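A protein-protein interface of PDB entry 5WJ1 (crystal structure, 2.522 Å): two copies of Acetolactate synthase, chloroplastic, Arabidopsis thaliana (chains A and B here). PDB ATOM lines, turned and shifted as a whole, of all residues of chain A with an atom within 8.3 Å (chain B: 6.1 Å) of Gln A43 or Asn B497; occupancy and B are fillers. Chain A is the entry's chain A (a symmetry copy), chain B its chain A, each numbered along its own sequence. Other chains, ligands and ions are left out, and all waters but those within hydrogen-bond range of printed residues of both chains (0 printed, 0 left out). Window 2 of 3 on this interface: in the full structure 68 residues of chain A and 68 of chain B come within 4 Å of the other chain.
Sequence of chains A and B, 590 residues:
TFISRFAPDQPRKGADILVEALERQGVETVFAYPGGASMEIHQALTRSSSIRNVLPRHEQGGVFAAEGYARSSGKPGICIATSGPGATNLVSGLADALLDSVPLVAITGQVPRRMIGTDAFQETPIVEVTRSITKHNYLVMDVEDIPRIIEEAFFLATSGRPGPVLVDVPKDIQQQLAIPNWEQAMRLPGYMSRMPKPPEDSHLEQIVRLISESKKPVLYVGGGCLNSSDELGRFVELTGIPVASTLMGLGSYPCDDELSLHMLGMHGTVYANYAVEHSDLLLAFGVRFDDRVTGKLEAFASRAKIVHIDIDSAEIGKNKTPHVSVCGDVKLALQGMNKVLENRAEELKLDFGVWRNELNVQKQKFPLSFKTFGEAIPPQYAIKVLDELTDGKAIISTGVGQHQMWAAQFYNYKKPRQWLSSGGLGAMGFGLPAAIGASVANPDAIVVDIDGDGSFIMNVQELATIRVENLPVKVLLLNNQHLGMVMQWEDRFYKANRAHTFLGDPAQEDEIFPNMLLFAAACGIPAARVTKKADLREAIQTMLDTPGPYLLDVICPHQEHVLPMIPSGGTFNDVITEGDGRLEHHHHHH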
ATOM      1  N   ARG A   5      13.715  12.078 -16.575  1.00  0.00           N
ATOM      2  CA  ARG A   5      15.122  12.273 -16.243  1.00  0.00           C
ATOM      3  C   ARG A   5      16.003  11.889 -17.426  1.00  0.00           C
ATOM      4  O   ARG A   5      17.229  11.963 -17.353  1.00  0.00           O
ATOM      5  CB  ARG A   5      15.508  11.452 -15.010  1.00  0.00           C
ATOM      6  CG  ARG A   5      14.645  11.721 -13.786  1.00  0.00           C
ATOM      7  CD  ARG A   5      15.063  10.845 -12.612  1.00  0.00           C
ATOM      8  NE  ARG A   5      14.977   9.423 -12.934  1.00  0.00           N
ATOM      9  CZ  ARG A   5      13.928   8.657 -12.658  1.00  0.00           C
ATOM     10  NH1 ARG A   5      12.872   9.176 -12.049  1.00  0.00           N
ATOM     11  NH2 ARG A   5      13.934   7.371 -12.986  1.00  0.00           N
ATOM     12  N   LYS A  13      17.744   1.665 -19.643  1.00  0.00           N
ATOM     13  CA  LYS A  13      17.372   0.324 -19.191  1.00  0.00           C
ATOM     14  C   LYS A  13      15.864   0.145 -19.034  1.00  0.00           C
ATOM     15  O   LYS A  13      15.147   1.089 -18.697  1.00  0.00           O
ATOM     16  CB  LYS A  13      18.054   0.000 -17.859  1.00  0.00           C
ATOM     17  CG  LYS A  13      19.521  -0.376 -17.965  1.00  0.00           C
ATOM     18  CD  LYS A  13      20.089  -0.652 -16.582  1.00  0.00           C
ATOM     19  CE  LYS A  13      21.582  -0.921 -16.628  1.00  0.00           C
ATOM     20  NZ  LYS A  13      22.106  -1.321 -15.292  1.00  0.00           N
ATOM     21  N   ALA A  15      14.425  -1.371 -16.734  1.00  0.00           N
ATOM     22  CA  ALA A  15      14.134  -1.117 -15.330  1.00  0.00           C
ATOM     23  C   ALA A  15      13.866   0.364 -15.088  1.00  0.00           C
ATOM     24  O   ALA A  15      13.017   0.721 -14.271  1.00  0.00           O
ATOM     25  CB  ALA A  15      15.276  -1.599 -14.457  1.00  0.00           C
ATOM     26  N   ASP A  16      14.589   1.223 -15.799  1.00  0.00           N
ATOM     27  CA  ASP A  16      14.376   2.661 -15.684  1.00  0.00           C
ATOM     28  C   ASP A  16      13.091   3.073 -16.394  1.00  0.00           C
ATOM     29  O   ASP A  16      12.462   4.068 -16.034  1.00  0.00           O
ATOM     30  CB  ASP A  16      15.569   3.439 -16.248  1.00  0.00           C
ATOM     31  CG  ASP A  16      16.776   3.407 -15.327  1.00  0.00           C
ATOM     32  OD1 ASP A  16      16.783   4.153 -14.324  1.00  0.00           O
ATOM     33  OD2 ASP A  16      17.720   2.639 -15.606  1.00  0.00           O
ATOM     34  N   VAL A  19      10.275   2.144 -13.821  1.00  0.00           N
ATOM     35  CA  VAL A  19      10.172   3.090 -12.714  1.00  0.00           C
ATOM     36  C   VAL A  19       9.531   4.403 -13.173  1.00  0.00           C
ATOM     37  O   VAL A  19       8.687   4.964 -12.474  1.00  0.00           O
ATOM     38  CB  VAL A  19      11.548   3.368 -12.074  1.00  0.00           C
ATOM     39  CG1 VAL A  19      11.474   4.551 -11.115  1.00  0.00           C
ATOM     40  CG2 VAL A  19      12.047   2.129 -11.349  1.00  0.00           C
ATOM     41  N   PRO A  34      14.413  -6.341  -2.130  1.00  0.00           N
ATOM     42  CA  PRO A  34      15.350  -6.654  -3.216  1.00  0.00           C
ATOM     43  C   PRO A  34      15.772  -8.119  -3.305  1.00  0.00           C
ATOM     44  O   PRO A  34      15.763  -8.853  -2.315  1.00  0.00           O
ATOM     45  CB  PRO A  34      16.558  -5.775  -2.886  1.00  0.00           C
ATOM     46  CG  PRO A  34      16.516  -5.635  -1.412  1.00  0.00           C
ATOM     47  CD  PRO A  34      15.061  -5.581  -1.045  1.00  0.00           C
ATOM     48  N   SER A  38      15.457  -8.797  -9.270  1.00  0.00           N
ATOM     49  CA  SER A  38      14.860  -7.461  -9.260  1.00  0.00           C
ATOM     50  C   SER A  38      15.861  -6.364  -8.887  1.00  0.00           C
ATOM     51  O   SER A  38      15.466  -5.229  -8.615  1.00  0.00           O
ATOM     52  CB  SER A  38      13.662  -7.415  -8.304  1.00  0.00           C
ATOM     53  OG  SER A  38      14.057  -7.601  -6.956  1.00  0.00           O
ATOM     54  N   MET A  39      17.148  -6.702  -8.889  1.00  0.00           N
ATOM     55  CA  MET A  39      18.202  -5.747  -8.539  1.00  0.00           C
ATOM     56  C   MET A  39      18.198  -4.508  -9.424  1.00  0.00           C
ATOM     57  O   MET A  39      18.370  -3.390  -8.937  1.00  0.00           O
ATOM     58  CB  MET A  39      19.577  -6.411  -8.624  1.00  0.00           C
ATOM     59  CG  MET A  39      19.953  -7.232  -7.413  1.00  0.00           C
ATOM     60  SD  MET A  39      21.713  -7.592  -7.409  1.00  0.00           S
ATOM     61  CE  MET A  39      22.376  -6.004  -6.913  1.00  0.00           C
ATOM     62  N   GLU A  40      18.021  -4.716 -10.725  1.00  0.00           N
ATOM     63  CA  GLU A  40      18.014  -3.619 -11.685  1.00  0.00           C
ATOM     64  C   GLU A  40      16.880  -2.642 -11.391  1.00  0.00           C
ATOM     65  O   GLU A  40      17.037  -1.430 -11.536  1.00  0.00           O
ATOM     66  CB  GLU A  40      17.893  -4.160 -13.111  1.00  0.00           C
ATOM     67  CG  GLU A  40      19.063  -5.028 -13.552  1.00  0.00           C
ATOM     68  CD  GLU A  40      20.257  -4.216 -14.018  1.00  0.00           C
ATOM     69  OE1 GLU A  40      20.110  -2.987 -14.198  1.00  0.00           O
ATOM     70  OE2 GLU A  40      21.343  -4.806 -14.210  1.00  0.00           O
ATOM     71  N   ILE A  41      15.740  -3.178 -10.970  1.00  0.00           N
ATOM     72  CA  ILE A  41      14.593  -2.350 -10.623  1.00  0.00           C
ATOM     73  C   ILE A  41      14.903  -1.503  -9.392  1.00  0.00           C
ATOM     74  O   ILE A  41      14.550  -0.323  -9.330  1.00  0.00           O
ATOM     75  CB  ILE A  41      13.335  -3.209 -10.368  1.00  0.00           C
ATOM     76  CG1 ILE A  41      12.921  -3.930 -11.653  1.00  0.00           C
ATOM     77  CG2 ILE A  41      12.183  -2.351  -9.851  1.00  0.00           C
ATOM     78  CD1 ILE A  41      11.723  -4.841 -11.491  1.00  0.00           C
ATOM     79  N   HIS A  42      15.583  -2.103  -8.420  1.00  0.00           N
ATOM     80  CA  HIS A  42      15.936  -1.390  -7.200  1.00  0.00           C
ATOM     81  C   HIS A  42      16.988  -0.314  -7.460  1.00  0.00           C
ATOM     82  O   HIS A  42      16.948   0.757  -6.852  1.00  0.00           O
ATOM     83  CB  HIS A  42      16.417  -2.369  -6.129  1.00  0.00           C
ATOM     84  CG  HIS A  42      15.301  -3.021  -5.377  1.00  0.00           C
ATOM     85  ND1 HIS A  42      14.940  -2.639  -4.102  1.00  0.00           N
ATOM     86  CD2 HIS A  42      14.447  -4.013  -5.728  1.00  0.00           C
ATOM     87  CE1 HIS A  42      13.922  -3.376  -3.696  1.00  0.00           C
ATOM     88  NE2 HIS A  42      13.601  -4.216  -4.664  1.00  0.00           N
ATOM     89  N   GLN A  43      17.921  -0.596  -8.365  1.00  0.00           N
ATOM     90  CA  GLN A  43      18.906   0.396  -8.776  1.00  0.00           C
ATOM     91  C   GLN A  43      18.211   1.591  -9.427  1.00  0.00           C
ATOM     92  O   GLN A  43      18.562   2.742  -9.168  1.00  0.00           O
ATOM     93  CB  GLN A  43      19.930  -0.220  -9.736  1.00  0.00           C
ATOM     94  CG  GLN A  43      20.895  -1.196  -9.074  1.00  0.00           C
ATOM     95  CD  GLN A  43      21.797  -0.525  -8.056  1.00  0.00           C
ATOM     96  OE1 GLN A  43      22.335   0.555  -8.303  1.00  0.00           O
ATOM     97  NE2 GLN A  43      21.958  -1.157  -6.897  1.00  0.00           N
ATOM     98  N   ALA A  44      17.213   1.307 -10.260  1.00  0.00           N
ATOM     99  CA  ALA A  44      16.454   2.355 -10.937  1.00  0.00           C
ATOM    100  C   ALA A  44      15.604   3.159  -9.954  1.00  0.00           C
ATOM    101  O   ALA A  44      15.357   4.349 -10.165  1.00  0.00           O
ATOM    102  CB  ALA A  44      15.579   1.753 -12.023  1.00  0.00           C
ATOM    103  N   LEU A  45      15.157   2.508  -8.885  1.00  0.00           N
ATOM    104  CA  LEU A  45      14.373   3.179  -7.854  1.00  0.00           C
ATOM    105  C   LEU A  45      15.182   4.268  -7.145  1.00  0.00           C
ATOM    106  O   LEU A  45      14.649   5.328  -6.821  1.00  0.00           O
ATOM    107  CB  LEU A  45      13.852   2.167  -6.833  1.00  0.00           C
ATOM    108  CG  LEU A  45      12.571   1.414  -7.204  1.00  0.00           C
ATOM    109  CD1 LEU A  45      12.192   0.434  -6.108  1.00  0.00           C
ATOM    110  CD2 LEU A  45      11.436   2.394  -7.464  1.00  0.00           C
ATOM    111  N   THR A  46      16.467   4.008  -6.915  1.00  0.00           N
ATOM    112  CA  THR A  46      17.323   4.981  -6.238  1.00  0.00           C
ATOM    113  C   THR A  46      17.541   6.216  -7.107  1.00  0.00           C
ATOM    114  O   THR A  46      17.836   7.298  -6.596  1.00  0.00           O
ATOM    115  CB  THR A  46      18.706   4.390  -5.865  1.00  0.00           C
ATOM    116  OG1 THR A  46      19.448   4.089  -7.055  1.00  0.00           O
ATOM    117  CG2 THR A  46      18.550   3.128  -5.029  1.00  0.00           C
ATOM    118  N   ARG A  47      17.394   6.052  -8.419  1.00  0.00           N
ATOM    119  CA  ARG A  47      17.561   7.163  -9.350  1.00  0.00           C
ATOM    120  C   ARG A  47      16.305   8.023  -9.439  1.00  0.00           C
ATOM    121  O   ARG A  47      16.325   9.095 -10.041  1.00  0.00           O
ATOM    122  CB  ARG A  47      17.941   6.644 -10.738  1.00  0.00           C
ATOM    123  CG  ARG A  47      19.289   5.944 -10.781  1.00  0.00           C
ATOM    124  CD  ARG A  47      19.733   5.668 -12.209  1.00  0.00           C
ATOM    125  NE  ARG A  47      19.163   4.429 -12.729  1.00  0.00           N
ATOM    126  CZ  ARG A  47      19.736   3.236 -12.602  1.00  0.00           C
ATOM    127  NH1 ARG A  47      19.153   2.157 -13.108  1.00  0.00           N
ATOM    128  NH2 ARG A  47      20.894   3.123 -11.966  1.00  0.00           N
ATOM    129  N   SER A  48      15.217   7.548  -8.842  1.00  0.00           N
ATOM    130  CA  SER A  48      13.978   8.316  -8.782  1.00  0.00           C
ATOM    131  C   SER A  48      13.972   9.246  -7.574  1.00  0.00           C
ATOM    132  O   SER A  48      14.339   8.846  -6.469  1.00  0.00           O
ATOM    133  CB  SER A  48      12.764   7.387  -8.732  1.00  0.00           C
ATOM    134  OG  SER A  48      11.581   8.107  -8.429  1.00  0.00           O
ATOM    135  N   GLN A 174      14.780  -6.097 -17.914  1.00  0.00           N
ATOM    136  CA  GLN A 174      15.162  -4.962 -17.077  1.00  0.00           C
ATOM    137  C   GLN A 174      16.490  -4.352 -17.520  1.00  0.00           C
ATOM    138  O   GLN A 174      16.736  -3.164 -17.316  1.00  0.00           O
ATOM    139  CB  GLN A 174      15.262  -5.383 -15.608  1.00  0.00           C
ATOM    140  CG  GLN A 174      14.051  -6.123 -15.071  1.00  0.00           C
ATOM    141  CD  GLN A 174      14.274  -6.656 -13.666  1.00  0.00           C
ATOM    142  OE1 GLN A 174      15.092  -6.126 -12.913  1.00  0.00           O
ATOM    143  NE2 GLN A 174      13.547  -7.709 -13.309  1.00  0.00           N
ATOM    144  N   GLU B 490      25.989  -5.640  -5.546  1.00  0.00           N
ATOM    145  CA  GLU B 490      26.028  -4.186  -5.685  1.00  0.00           C
ATOM    146  C   GLU B 490      27.472  -3.697  -5.787  1.00  0.00           C
ATOM    147  O   GLU B 490      27.790  -2.840  -6.609  1.00  0.00           O
ATOM    148  CB  GLU B 490      25.323  -3.501  -4.508  1.00  0.00           C
ATOM    149  CG  GLU B 490      23.803  -3.630  -4.514  1.00  0.00           C
ATOM    150  CD  GLU B 490      23.153  -3.053  -3.261  1.00  0.00           C
ATOM    151  OE1 GLU B 490      23.846  -2.925  -2.229  1.00  0.00           O
ATOM    152  OE2 GLU B 490      21.947  -2.725  -3.311  1.00  0.00           O
ATOM    153  N   ASP B 491      28.340  -4.255  -4.947  1.00  0.00           N
ATOM    154  CA  ASP B 491      29.756  -3.893  -4.933  1.00  0.00           C
ATOM    155  C   ASP B 491      30.451  -4.261  -6.239  1.00  0.00           C
ATOM    156  O   ASP B 491      31.168  -3.447  -6.822  1.00  0.00           O
ATOM    157  CB  ASP B 491      30.479  -4.576  -3.765  1.00  0.00           C
ATOM    158  CG  ASP B 491      30.006  -4.087  -2.411  1.00  0.00           C
ATOM    159  OD1 ASP B 491      29.456  -2.967  -2.334  1.00  0.00           O
ATOM    160  OD2 ASP B 491      30.188  -4.825  -1.421  1.00  0.00           O
ATOM    161  N   TYR B 494      27.537  -2.905  -9.504  1.00  0.00           N
ATOM    162  CA  TYR B 494      26.786  -1.651  -9.504  1.00  0.00           C
ATOM    163  C   TYR B 494      27.509  -0.544  -8.738  1.00  0.00           C
ATOM    164  O   TYR B 494      26.871   0.355  -8.180  1.00  0.00           O
ATOM    165  CB  TYR B 494      25.387  -1.866  -8.925  1.00  0.00           C
ATOM    166  CG  TYR B 494      24.550  -2.845  -9.720  1.00  0.00           C
ATOM    167  CD1 TYR B 494      23.797  -2.425 -10.808  1.00  0.00           C
ATOM    168  CD2 TYR B 494      24.517  -4.192  -9.381  1.00  0.00           C
ATOM    169  CE1 TYR B 494      23.033  -3.317 -11.537  1.00  0.00           C
ATOM    170  CE2 TYR B 494      23.755  -5.093 -10.103  1.00  0.00           C
ATOM    171  CZ  TYR B 494      23.016  -4.650 -11.180  1.00  0.00           C
ATOM    172  OH  TYR B 494      22.258  -5.542 -11.902  1.00  0.00           O
ATOM    173  N   LYS B 495      28.839  -0.619  -8.726  1.00  0.00           N
ATOM    174  CA  LYS B 495      29.688   0.408  -8.126  1.00  0.00           C
ATOM    175  C   LYS B 495      29.323   0.693  -6.672  1.00  0.00           C
ATOM    176  O   LYS B 495      29.381   1.839  -6.229  1.00  0.00           O
ATOM    177  CB  LYS B 495      29.609   1.702  -8.941  1.00  0.00           C
ATOM    178  CG  LYS B 495      30.007   1.544 -10.398  1.00  0.00           C
ATOM    179  CD  LYS B 495      29.882   2.858 -11.151  1.00  0.00           C
ATOM    180  CE  LYS B 495      30.401   2.731 -12.574  1.00  0.00           C
ATOM    181  NZ  LYS B 495      31.843   2.357 -12.609  1.00  0.00           N
ATOM    182  N   ALA B 496      28.935  -0.356  -5.952  1.00  0.00           N
ATOM    183  CA  ALA B 496      28.572  -0.269  -4.538  1.00  0.00           C
ATOM    184  C   ALA B 496      27.421   0.703  -4.263  1.00  0.00           C
ATOM    185  O   ALA B 496      27.323   1.261  -3.169  1.00  0.00           O
ATOM    186  CB  ALA B 496      29.790   0.116  -3.705  1.00  0.00           C
ATOM    187  N   ASN B 497      26.550   0.901  -5.248  1.00  0.00           N
ATOM    188  CA  ASN B 497      25.373   1.739  -5.046  1.00  0.00           C
ATOM    189  C   ASN B 497      24.305   0.989  -4.260  1.00  0.00           C
ATOM    190  O   ASN B 497      23.660   0.081  -4.783  1.00  0.00           O
ATOM    191  CB  ASN B 497      24.803   2.213  -6.382  1.00  0.00           C
ATOM    192  CG  ASN B 497      23.639   3.174  -6.208  1.00  0.00           C
ATOM    193  OD1 ASN B 497      23.802   4.267  -5.667  1.00  0.00           O
ATOM    194  ND2 ASN B 497      22.458   2.768  -6.662  1.00  0.00           N
ATOM    195  N   ARG B 498      24.121   1.372  -3.001  1.00  0.00           N
ATOM    196  CA  ARG B 498      23.178   0.686  -2.122  1.00  0.00           C
ATOM    197  C   ARG B 498      21.729   0.928  -2.529  1.00  0.00           C
ATOM    198  O   ARG B 498      21.290   2.070  -2.659  1.00  0.00           O
ATOM    199  CB  ARG B 498      23.386   1.128  -0.672  1.00  0.00           C
ATOM    200  CG  ARG B 498      24.749   0.772  -0.108  1.00  0.00           C
ATOM    201  CD  ARG B 498      24.828  -0.698   0.270  1.00  0.00           C
ATOM    202  NE  ARG B 498      26.193  -1.080   0.618  1.00  0.00           N
ATOM    203  CZ  ARG B 498      27.034  -1.677  -0.219  1.00  0.00           C
ATOM    204  NH1 ARG B 498      26.643  -1.979  -1.450  1.00  0.00           N
ATOM    205  NH2 ARG B 498      28.261  -1.985   0.178  1.00  0.00           N
ATOM    206  N   ALA B 499      20.994  -0.158  -2.728  1.00  0.00           N
ATOM    207  CA  ALA B 499      19.570  -0.077  -3.023  1.00  0.00           C
ATOM    208  C   ALA B 499      18.781  -0.927  -2.032  1.00  0.00           C
ATOM    209  O   ALA B 499      18.396  -2.058  -2.334  1.00  0.00           O
ATOM    210  CB  ALA B 499      19.291  -0.516  -4.450  1.00  0.00           C
ATOM    211  N   HIS B 500      18.563  -0.367  -0.844  1.00  0.00           N
ATOM    212  CA  HIS B 500      17.746  -0.980   0.203  1.00  0.00           C
ATOM    213  C   HIS B 500      18.291  -2.330   0.671  1.00  0.00           C
ATOM    214  O   HIS B 500      17.546  -3.304   0.780  1.00  0.00           O
ATOM    215  CB  HIS B 500      16.298  -1.138  -0.281  1.00  0.00           C
ATOM    216  CG  HIS B 500      15.856  -0.051  -1.210  1.00  0.00           C
ATOM    217  ND1 HIS B 500      15.705  -0.248  -2.565  1.00  0.00           N
ATOM    218  CD2 HIS B 500      15.567   1.254  -0.984  1.00  0.00           C
ATOM    219  CE1 HIS B 500      15.325   0.883  -3.133  1.00  0.00           C
ATOM    220  NE2 HIS B 500      15.236   1.810  -2.196  1.00  0.00           N
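No position is printed for both chains.
His B500 touches Pro A34 (O to CG, 3.4 Å). Met A39 touches Glu B490. Met A39 touches Tyr B494. His A42 touches Ala B499. Glu B490 touches Gln A43. Tyr B494 touches Gln A43 (CD1 to CG, 3.6 Å). CB of Ala B499 touches NE2 of Gln A43 (3.7 Å). Thr A46 touches Arg B498. CB of Ala B499 touches CG2 of Thr A46 (3.8 Å).
Arg A5 touches none of the printed residues of chain B. Of the printed residues of chain B, His A42 touches Ala B499 (3.6 Å) and His B500 (2.9 Å). Of the printed residues of chain A, Glu B490 touches Met A39 (3.7 Å) and Gln A43 (3.9 Å). Of chain A, only Gln A43 (2.8 Å) and Thr A46 (3.3 Å) come within 4 Å of Asn B497. Of the printed residues of chain A, Arg B498 touches Thr A46. The nearest residue of chain A that does not touch Asn B497 is Arg A47 (5.5 Å).
The side-chain amino group of Lys A13 is in salt-bridge range of the side-chain carboxylate of Glu A40, 2.8 Å away. O of Glu B490 sits at hydrogen-bond distance from N of Ala B496 (2.8 Å). NH2 of Arg B498 lies within salt-bridge range of OD1 of Asp B491 (2.9 Å). The side-chain carboxylate (OE2) of Glu B490 sits at hydrogen-bond distance from the backbone NH (N) of Ala B499. The backbone carbonyl oxygen of Gln A43 is in hydrogen-bond range of the side-chain hydroxyl of Thr A46 (2.7 Å). The backbone carbonyl oxygen (O) of Glu B490 is in hydrogen-bond range of the backbone NH (N) of Lys B495 (3.2 Å).
Hydrophobic or aromatic side chains of chain A within 4 Å of the printed part of chain B: Pro A34, Met A39 and His A42. Hydrophobic or aromatic side chains of chain B that line the printed part of chain A: Tyr B494, Ala B499 and His B500.
ND1 of His B500 is in hydrogen-bond range of ND1 of His A42 (2.9 Å). The side-chain carboxylate (OE2) of Glu A40 is in hydrogen-bond range of the side-chain hydroxyl (OH) of Tyr B494, at 2.6 Å. ND2 of Asn B497 sits at hydrogen-bond distance from OG1 of Thr A46 (3.3 Å). The side-chain amide nitrogen of Asn B497 is in hydrogen-bond range of the side-chain amide oxygen of Gln A43 (2.8 Å).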
